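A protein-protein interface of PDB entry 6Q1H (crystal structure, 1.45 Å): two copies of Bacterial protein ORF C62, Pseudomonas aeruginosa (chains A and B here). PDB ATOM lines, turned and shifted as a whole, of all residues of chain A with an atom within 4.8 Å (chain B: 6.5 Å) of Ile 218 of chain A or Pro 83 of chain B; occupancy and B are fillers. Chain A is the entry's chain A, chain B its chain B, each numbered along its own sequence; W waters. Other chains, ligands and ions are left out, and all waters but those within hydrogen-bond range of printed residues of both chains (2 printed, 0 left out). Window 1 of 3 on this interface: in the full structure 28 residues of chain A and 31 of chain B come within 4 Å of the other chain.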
ATOM      1  N   TYR A  49     -16.871  17.569 -14.127  1.00  0.00           N
ATOM      2  CA  TYR A  49     -17.364  18.655 -14.963  1.00  0.00           C
ATOM      3  C   TYR A  49     -17.111  18.481 -16.458  1.00  0.00           C
ATOM      4  O   TYR A  49     -17.915  18.964 -17.272  1.00  0.00           O
ATOM      5  CB  TYR A  49     -16.802  19.994 -14.473  1.00  0.00           C
ATOM      6  CG  TYR A  49     -17.483  20.468 -13.207  1.00  0.00           C
ATOM      7  CD1 TYR A  49     -18.764  20.989 -13.253  1.00  0.00           C
ATOM      8  CD2 TYR A  49     -16.855  20.369 -11.968  1.00  0.00           C
ATOM      9  CE1 TYR A  49     -19.422  21.394 -12.103  1.00  0.00           C
ATOM     10  CE2 TYR A  49     -17.488  20.797 -10.820  1.00  0.00           C
ATOM     11  CZ  TYR A  49     -18.777  21.301 -10.888  1.00  0.00           C
ATOM     12  OH  TYR A  49     -19.476  21.710  -9.770  1.00  0.00           O
ATOM     13  N   LEU A  50     -16.036  17.831 -16.886  1.00  0.00           N
ATOM     14  CA  LEU A  50     -15.848  17.709 -18.318  1.00  0.00           C
ATOM     15  C   LEU A  50     -16.988  16.878 -18.913  1.00  0.00           C
ATOM     16  O   LEU A  50     -17.510  15.954 -18.282  1.00  0.00           O
ATOM     17  CB  LEU A  50     -14.526  17.041 -18.701  1.00  0.00           C
ATOM     18  CG  LEU A  50     -13.222  17.811 -18.532  1.00  0.00           C
ATOM     19  CD1 LEU A  50     -12.044  16.888 -18.929  1.00  0.00           C
ATOM     20  CD2 LEU A  50     -13.194  19.106 -19.290  1.00  0.00           C
ATOM     21  N   PRO A  51     -17.368  17.161 -20.165  1.00  0.00           N
ATOM     22  CA  PRO A  51     -18.260  16.247 -20.892  1.00  0.00           C
ATOM     23  C   PRO A  51     -17.741  14.816 -20.822  1.00  0.00           C
ATOM     24  O   PRO A  51     -16.542  14.578 -20.832  1.00  0.00           O
ATOM     25  CB  PRO A  51     -18.214  16.792 -22.322  1.00  0.00           C
ATOM     26  CG  PRO A  51     -17.996  18.292 -22.124  1.00  0.00           C
ATOM     27  CD  PRO A  51     -17.059  18.373 -20.928  1.00  0.00           C
ATOM     28  N   LEU A 214     -11.343  25.666 -16.337  1.00  0.00           N
ATOM     29  CA  LEU A 214     -12.227  24.612 -16.817  1.00  0.00           C
ATOM     30  C   LEU A 214     -12.969  25.044 -18.061  1.00  0.00           C
ATOM     31  O   LEU A 214     -13.053  24.279 -19.036  1.00  0.00           O
ATOM     32  CB  LEU A 214     -13.231  24.285 -15.713  1.00  0.00           C
ATOM     33  CG  LEU A 214     -14.300  23.246 -16.032  1.00  0.00           C
ATOM     34  CD1 LEU A 214     -13.630  21.909 -16.240  1.00  0.00           C
ATOM     35  CD2 LEU A 214     -15.262  23.206 -14.830  1.00  0.00           C
ATOM     36  N   PHE A 215     -13.493  26.268 -18.065  1.00  0.00           N
ATOM     37  CA  PHE A 215     -14.263  26.739 -19.209  1.00  0.00           C
ATOM     38  C   PHE A 215     -13.358  26.918 -20.425  1.00  0.00           C
ATOM     39  O   PHE A 215     -13.740  26.559 -21.537  1.00  0.00           O
ATOM     40  CB  PHE A 215     -14.979  28.037 -18.855  1.00  0.00           C
ATOM     41  CG  PHE A 215     -16.230  27.854 -18.033  1.00  0.00           C
ATOM     42  CD1 PHE A 215     -16.610  26.619 -17.568  1.00  0.00           C
ATOM     43  CD2 PHE A 215     -17.011  28.954 -17.721  1.00  0.00           C
ATOM     44  CE1 PHE A 215     -17.779  26.474 -16.801  1.00  0.00           C
ATOM     45  CE2 PHE A 215     -18.170  28.814 -16.958  1.00  0.00           C
ATOM     46  CZ  PHE A 215     -18.553  27.588 -16.535  1.00  0.00           C
ATOM     47  N   LYS A 216     -12.153  27.473 -20.233  1.00  0.00           N
ATOM     48  CA  LYS A 216     -11.231  27.602 -21.359  1.00  0.00           C
ATOM     49  C   LYS A 216     -10.848  26.226 -21.905  1.00  0.00           C
ATOM     50  O   LYS A 216     -10.764  26.039 -23.124  1.00  0.00           O
ATOM     51  CB  LYS A 216      -9.995  28.435 -20.965  1.00  0.00           C
ATOM     52  CG  LYS A 216      -9.028  28.738 -22.094  1.00  0.00           C
ATOM     53  CD  LYS A 216      -9.711  29.404 -23.283  1.00  0.00           C
ATOM     54  CE  LYS A 216      -8.697  29.882 -24.327  1.00  0.00           C
ATOM     55  NZ  LYS A 216      -9.339  30.416 -25.565  1.00  0.00           N
ATOM     56  N   LEU A 217     -10.619  25.258 -21.018  1.00  0.00           N
ATOM     57  CA  LEU A 217     -10.236  23.928 -21.465  1.00  0.00           C
ATOM     58  C   LEU A 217     -11.345  23.299 -22.303  1.00  0.00           C
ATOM     59  O   LEU A 217     -11.098  22.716 -23.356  1.00  0.00           O
ATOM     60  CB  LEU A 217      -9.930  23.038 -20.260  1.00  0.00           C
ATOM     61  CG  LEU A 217      -9.643  21.577 -20.558  1.00  0.00           C
ATOM     62  CD1 LEU A 217      -8.416  21.437 -21.505  1.00  0.00           C
ATOM     63  CD2 LEU A 217      -9.406  20.775 -19.290  1.00  0.00           C
ATOM     64  N   ILE A 218     -12.587  23.395 -21.832  1.00  0.00           N
ATOM     65  CA  ILE A 218     -13.698  22.830 -22.591  1.00  0.00           C
ATOM     66  C   ILE A 218     -13.784  23.483 -23.962  1.00  0.00           C
ATOM     67  O   ILE A 218     -13.924  22.807 -24.984  1.00  0.00           O
ATOM     68  CB  ILE A 218     -15.013  22.985 -21.812  1.00  0.00           C
ATOM     69  CG1 ILE A 218     -15.015  22.107 -20.564  1.00  0.00           C
ATOM     70  CG2 ILE A 218     -16.227  22.640 -22.721  1.00  0.00           C
ATOM     71  CD1 ILE A 218     -16.153  22.363 -19.596  1.00  0.00           C
ATOM     72  N   ALA A 219     -13.697  24.817 -24.006  1.00  0.00           N
ATOM     73  CA  ALA A 219     -13.783  25.534 -25.274  1.00  0.00           C
ATOM     74  C   ALA A 219     -12.642  25.152 -26.220  1.00  0.00           C
ATOM     75  O   ALA A 219     -12.867  24.951 -27.428  1.00  0.00           O
ATOM     76  CB  ALA A 219     -13.754  27.044 -25.027  1.00  0.00           C
ATOM     77  N   GLN A 220     -11.410  25.042 -25.698  1.00  0.00           N
ATOM     78  CA  GLN A 220     -10.292  24.641 -26.554  1.00  0.00           C
ATOM     79  C   GLN A 220     -10.479  23.208 -27.052  1.00  0.00           C
ATOM     80  O   GLN A 220     -10.250  22.915 -28.231  1.00  0.00           O
ATOM     81  CB  GLN A 220      -8.970  24.717 -25.787  1.00  0.00           C
ATOM     82  CG  GLN A 220      -8.383  26.085 -25.532  1.00  0.00           C
ATOM     83  CD  GLN A 220      -7.074  26.006 -24.756  1.00  0.00           C
ATOM     84  OE1 GLN A 220      -6.892  25.105 -23.925  1.00  0.00           O
ATOM     85  NE2 GLN A 220      -6.154  26.939 -25.013  1.00  0.00           N
ATOM     86  N   LEU A 221     -10.921  22.315 -26.163  1.00  0.00           N
ATOM     87  CA  LEU A 221     -11.089  20.914 -26.536  1.00  0.00           C
ATOM     88  C   LEU A 221     -12.138  20.752 -27.634  1.00  0.00           C
ATOM     89  O   LEU A 221     -12.023  19.861 -28.473  1.00  0.00           O
ATOM     90  CB  LEU A 221     -11.492  20.084 -25.318  1.00  0.00           C
ATOM     91  CG  LEU A 221     -10.365  19.714 -24.329  1.00  0.00           C
ATOM     92  CD1 LEU A 221     -10.971  19.127 -23.075  1.00  0.00           C
ATOM     93  CD2 LEU A 221      -9.423  18.711 -24.934  1.00  0.00           C
ATOM     94  N   GLN A 222     -13.188  21.580 -27.615  1.00  0.00           N
ATOM     95  CA  GLN A 222     -14.244  21.443 -28.614  1.00  0.00           C
ATOM     96  C   GLN A 222     -13.667  21.495 -30.020  1.00  0.00           C
ATOM     97  O   GLN A 222     -14.171  20.821 -30.933  1.00  0.00           O
ATOM     98  CB  GLN A 222     -15.319  22.512 -28.454  1.00  0.00           C
ATOM     99  CG  GLN A 222     -16.290  22.185 -27.345  1.00  0.00           C
ATOM    100  CD  GLN A 222     -17.240  23.324 -27.044  1.00  0.00           C
ATOM    101  OE1 GLN A 222     -16.934  24.500 -27.262  1.00  0.00           O
ATOM    102  NE2 GLN A 222     -18.411  22.977 -26.507  1.00  0.00           N
ATOM    103  N   ASP B  78     -28.233  15.899 -21.760  1.00  0.00           N
ATOM    104  CA  ASP B  78     -26.958  15.382 -22.244  1.00  0.00           C
ATOM    105  C   ASP B  78     -25.838  15.631 -21.254  1.00  0.00           C
ATOM    106  O   ASP B  78     -25.766  16.705 -20.633  1.00  0.00           O
ATOM    107  CB  ASP B  78     -26.541  16.108 -23.524  1.00  0.00           C
ATOM    108  CG  ASP B  78     -25.121  15.765 -23.962  1.00  0.00           C
ATOM    109  OD1 ASP B  78     -24.901  14.629 -24.431  1.00  0.00           O
ATOM    110  OD2 ASP B  78     -24.221  16.642 -23.788  1.00  0.00           O
ATOM    111  N   ARG B  79     -24.951  14.636 -21.129  1.00  0.00           N
ATOM    112  CA  ARG B  79     -23.646  14.811 -20.482  1.00  0.00           C
ATOM    113  C   ARG B  79     -22.475  14.410 -21.356  1.00  0.00           C
ATOM    114  O   ARG B  79     -21.338  14.668 -20.974  1.00  0.00           O
ATOM    115  CB  ARG B  79     -23.551  14.030 -19.149  1.00  0.00           C
ATOM    116  CG  ARG B  79     -24.119  14.799 -18.002  1.00  0.00           C
ATOM    117  CD  ARG B  79     -23.132  15.834 -17.447  1.00  0.00           C
ATOM    118  NE  ARG B  79     -22.009  15.180 -16.774  1.00  0.00           N
ATOM    119  CZ  ARG B  79     -20.730  15.432 -16.999  1.00  0.00           C
ATOM    120  NH1 ARG B  79     -20.360  16.401 -17.838  1.00  0.00           N
ATOM    121  NH2 ARG B  79     -19.814  14.749 -16.310  1.00  0.00           N
ATOM    122  N   TYR B  81     -21.555  15.714 -24.177  1.00  0.00           N
ATOM    123  CA  TYR B  81     -21.017  16.923 -24.794  1.00  0.00           C
ATOM    124  C   TYR B  81     -21.215  18.159 -23.933  1.00  0.00           C
ATOM    125  O   TYR B  81     -20.944  19.287 -24.388  1.00  0.00           O
ATOM    126  CB  TYR B  81     -21.697  17.130 -26.156  1.00  0.00           C
ATOM    127  CG  TYR B  81     -21.483  15.973 -27.087  1.00  0.00           C
ATOM    128  CD1 TYR B  81     -20.277  15.817 -27.758  1.00  0.00           C
ATOM    129  CD2 TYR B  81     -22.472  15.034 -27.303  1.00  0.00           C
ATOM    130  CE1 TYR B  81     -20.063  14.741 -28.602  1.00  0.00           C
ATOM    131  CE2 TYR B  81     -22.249  13.932 -28.130  1.00  0.00           C
ATOM    132  CZ  TYR B  81     -21.044  13.829 -28.805  1.00  0.00           C
ATOM    133  OH  TYR B  81     -20.846  12.757 -29.632  1.00  0.00           O
ATOM    134  N   SER B  82     -21.750  18.001 -22.719  1.00  0.00           N
ATOM    135  CA  SER B  82     -22.146  19.139 -21.914  1.00  0.00           C
ATOM    136  C   SER B  82     -21.578  18.997 -20.514  1.00  0.00           C
ATOM    137  O   SER B  82     -21.623  17.905 -19.939  1.00  0.00           O
ATOM    138  CB  SER B  82     -23.681  19.193 -21.795  1.00  0.00           C
ATOM    139  OG  SER B  82     -24.301  19.189 -23.055  1.00  0.00           O
ATOM    140  N   PRO B  83     -21.039  20.066 -19.943  1.00  0.00           N
ATOM    141  CA  PRO B  83     -20.665  20.045 -18.535  1.00  0.00           C
ATOM    142  C   PRO B  83     -21.892  20.252 -17.665  1.00  0.00           C
ATOM    143  O   PRO B  83     -22.937  20.729 -18.111  1.00  0.00           O
ATOM    144  CB  PRO B  83     -19.736  21.265 -18.416  1.00  0.00           C
ATOM    145  CG  PRO B  83     -20.351  22.240 -19.403  1.00  0.00           C
ATOM    146  CD  PRO B  83     -20.868  21.404 -20.542  1.00  0.00           C
ATOM    147  N   PHE B  84     -21.758  19.872 -16.383  1.00  0.00           N
ATOM    148  CA  PHE B  84     -22.593  20.514 -15.374  1.00  0.00           C
ATOM    149  C   PHE B  84     -22.124  21.954 -15.189  1.00  0.00           C
ATOM    150  O   PHE B  84     -20.945  22.274 -15.396  1.00  0.00           O
ATOM    151  CB  PHE B  84     -22.451  19.817 -14.003  1.00  0.00           C
ATOM    152  CG  PHE B  84     -23.002  18.424 -13.950  1.00  0.00           C
ATOM    153  CD1 PHE B  84     -24.348  18.195 -14.123  1.00  0.00           C
ATOM    154  CD2 PHE B  84     -22.180  17.359 -13.734  1.00  0.00           C
ATOM    155  CE1 PHE B  84     -24.870  16.916 -14.076  1.00  0.00           C
ATOM    156  CE2 PHE B  84     -22.698  16.075 -13.669  1.00  0.00           C
ATOM    157  CZ  PHE B  84     -24.041  15.867 -13.838  1.00  0.00           C
ATOM    158  N   ILE B  85     -23.037  22.823 -14.759  1.00  0.00           N
ATOM    159  CA  ILE B  85     -22.629  24.149 -14.311  1.00  0.00           C
ATOM    160  C   ILE B  85     -22.203  24.102 -12.836  1.00  0.00           C
ATOM    161  O   ILE B  85     -21.226  24.748 -12.451  1.00  0.00           O
ATOM    162  CB  ILE B  85     -23.702  25.213 -14.583  1.00  0.00           C
ATOM    163  CG1 ILE B  85     -23.978  25.338 -16.083  1.00  0.00           C
ATOM    164  CG2 ILE B  85     -23.276  26.547 -13.986  1.00  0.00           C
ATOM    165  CD1 ILE B  85     -22.766  25.705 -16.914  1.00  0.00           C
ATOM    166  N   ILE B  93     -27.052  21.556 -10.973  1.00  0.00           N
ATOM    167  CA  ILE B  93     -27.541  22.585 -11.886  1.00  0.00           C
ATOM    168  C   ILE B  93     -26.897  22.331 -13.246  1.00  0.00           C
ATOM    169  O   ILE B  93     -25.663  22.275 -13.353  1.00  0.00           O
ATOM    170  CB  ILE B  93     -27.242  24.003 -11.389  1.00  0.00           C
ATOM    171  CG1 ILE B  93     -27.906  24.250 -10.034  1.00  0.00           C
ATOM    172  CG2 ILE B  93     -27.763  25.027 -12.416  1.00  0.00           C
ATOM    173  CD1 ILE B  93     -27.022  23.992  -8.874  1.00  0.00           C
ATOM    174  N   ILE B  94     -27.725  22.186 -14.282  1.00  0.00           N
ATOM    175  CA  ILE B  94     -27.292  21.854 -15.637  1.00  0.00           C
ATOM    176  C   ILE B  94     -27.509  23.068 -16.529  1.00  0.00           C
ATOM    177  O   ILE B  94     -28.412  23.880 -16.254  1.00  0.00           O
ATOM    178  CB  ILE B  94     -28.019  20.624 -16.205  1.00  0.00           C
ATOM    179  CG1 ILE B  94     -29.517  20.891 -16.271  1.00  0.00           C
ATOM    180  CG2 ILE B  94     -27.699  19.369 -15.372  1.00  0.00           C
ATOM    181  CD1 ILE B  94     -30.305  19.758 -16.933  1.00  0.00           C
ATOM    182  N   PRO B  95     -26.751  23.195 -17.611  1.00  0.00           N
ATOM    183  CA  PRO B  95     -26.963  24.293 -18.557  1.00  0.00           C
ATOM    184  C   PRO B  95     -28.154  24.012 -19.455  1.00  0.00           C
ATOM    185  O   PRO B  95     -28.444  22.866 -19.808  1.00  0.00           O
ATOM    186  CB  PRO B  95     -25.651  24.311 -19.361  1.00  0.00           C
ATOM    187  CG  PRO B  95     -25.194  22.910 -19.359  1.00  0.00           C
ATOM    188  CD  PRO B  95     -25.624  22.324 -18.005  1.00  0.00           C
ATOM    189  N   SER B  98     -28.049  21.606 -22.441  1.00  0.00           N
ATOM    190  CA  SER B  98     -28.006  20.161 -22.271  1.00  0.00           C
ATOM    191  C   SER B  98     -29.387  19.511 -22.275  1.00  0.00           C
ATOM    192  O   SER B  98     -29.447  18.270 -22.283  1.00  0.00           O
ATOM    193  CB  SER B  98     -27.304  19.833 -20.945  1.00  0.00           C
ATOM    194  OG  SER B  98     -28.154  20.097 -19.817  1.00  0.00           O
ATOM    195  N   ILE B 230     -22.648  23.667 -26.884  1.00  0.00           N
ATOM    196  CA  ILE B 230     -22.686  24.764 -25.920  1.00  0.00           C
ATOM    197  C   ILE B 230     -21.516  25.717 -26.097  1.00  0.00           C
ATOM    198  O   ILE B 230     -20.373  25.309 -26.346  1.00  0.00           O
ATOM    199  CB  ILE B 230     -22.727  24.169 -24.501  1.00  0.00           C
ATOM    200  CG1 ILE B 230     -22.908  25.256 -23.436  1.00  0.00           C
ATOM    201  CG2 ILE B 230     -21.470  23.348 -24.223  1.00  0.00           C
ATOM    202  CD1 ILE B 230     -23.116  24.697 -22.013  1.00  0.00           C
ATOM    203  N   VAL B 232     -19.536  27.495 -23.757  1.00  0.00           N
ATOM    204  CA  VAL B 232     -19.292  27.631 -22.332  1.00  0.00           C
ATOM    205  C   VAL B 232     -18.724  28.998 -21.971  1.00  0.00           C
ATOM    206  O   VAL B 232     -18.883  29.442 -20.835  1.00  0.00           O
ATOM    207  CB  VAL B 232     -18.395  26.528 -21.728  1.00  0.00           C
ATOM    208  CG1 VAL B 232     -19.035  25.205 -21.932  1.00  0.00           C
ATOM    209  CG2 VAL B 232     -16.998  26.547 -22.315  1.00  0.00           C
HETATM  210  O   HOH W   1     -19.594  20.213 -26.600  1.00  0.00           O
HETATM  211  O   HOH W   2     -17.399  26.617 -25.534  1.00  0.00           O
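The backbone carbonyl oxygen (O) of Leu 50 of chain A sits at hydrogen-bond distance from the guanidinium group (NH1) of Arg 79 of chain B (2.9 Å). O of Ile 230 of chain B sits at hydrogen-bond distance from NE2 of Gln 222 of chain A (3.1 Å).
OD2 of Asp 78 of chain B lies within hydrogen-bond range of N of Tyr 81 of chain B (2.8 Å). N of Ile 85 of chain B lies within hydrogen-bond range of O of Ile 93 of chain B, 3.0 Å away. The side-chain hydroxyl (OG) of Ser 82 of chain B lies within hydrogen-bond range of the side-chain carboxylate (OD2) of Asp 78 of chain B (2.7 Å). The guanidinium group of Arg 79 of chain B lies within hydrogen-bond range of the backbone carbonyl oxygen of Ser 82 of chain B (2.9 Å).
Among the printed residues, merely in contact across the chains: Tyr 49 of chain A with Arg 79 of chain B, Tyr 49 of chain A with Pro 83 of chain B, Tyr 49 of chain A with Phe 84 of chain B, Tyr 49 of chain A with Ile 85 of chain B, Pro 51 of chain A with Arg 79 of chain B, Pro 51 of chain A with Tyr 81 of chain B, Pro 51 of chain A with Ser 82 of chain B, Phe 215 of chain A with Val 232 of chain B, Ile 218 of chain A with Pro 83 of chain B and Ile 218 of chain A with Val 232 of chain B.
Of chain B, only Pro 83 and Val 232 come within 4 Å of Ile 218 of chain A. Of chain A, only Tyr 49 and Ile 218 come within 4 Å of Pro 83 of chain B. Printed residues of chain B within 4 Å of Leu 50 of chain A: Arg 79 (2.9 Å). Of the printed residues of chain A, Tyr 81 of chain B touches Pro 51. Leu 214 of chain A touches none of the printed residues of chain B. The nearest printed residue of chain A that does not touch Val 232 of chain B is Ala 219 of chain A (4.1 Å).
Along chain B the printed residues that touch a printed residue of chain A span positions 79 to 232. Printed residues of chain A that touch a printed residue of chain B: Tyr 49, Leu 50, Pro 51, Phe 215, Ile 218 and Gln 222. Hydrophobic or aromatic side chains of chain A that line the printed part of chain B: Tyr 49, Pro 51, Phe 215 and Ile 218. Among the printed residues, 12 pairs touch across the chains. Among the printed residues, no Asp or Glu carboxylate lies within 4 Å of a Lys or Arg side-chain nitrogen of the other chain.
No position is printed for both chains.
Water W1 lies within hydrogen-bond range of O of Tyr 81 of chain B (2.8 Å) and NE2 of Gln 222 of chain A (3.0 Å). Water W2 lies within hydrogen-bond range of the side-chain amide oxygen of Gln 222 of chain A (2.8 Å), the backbone NH of Val 232 of chain B (2.9 Å) and the backbone carbonyl oxygen of Ile 230 of chain B (3.3 Å).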
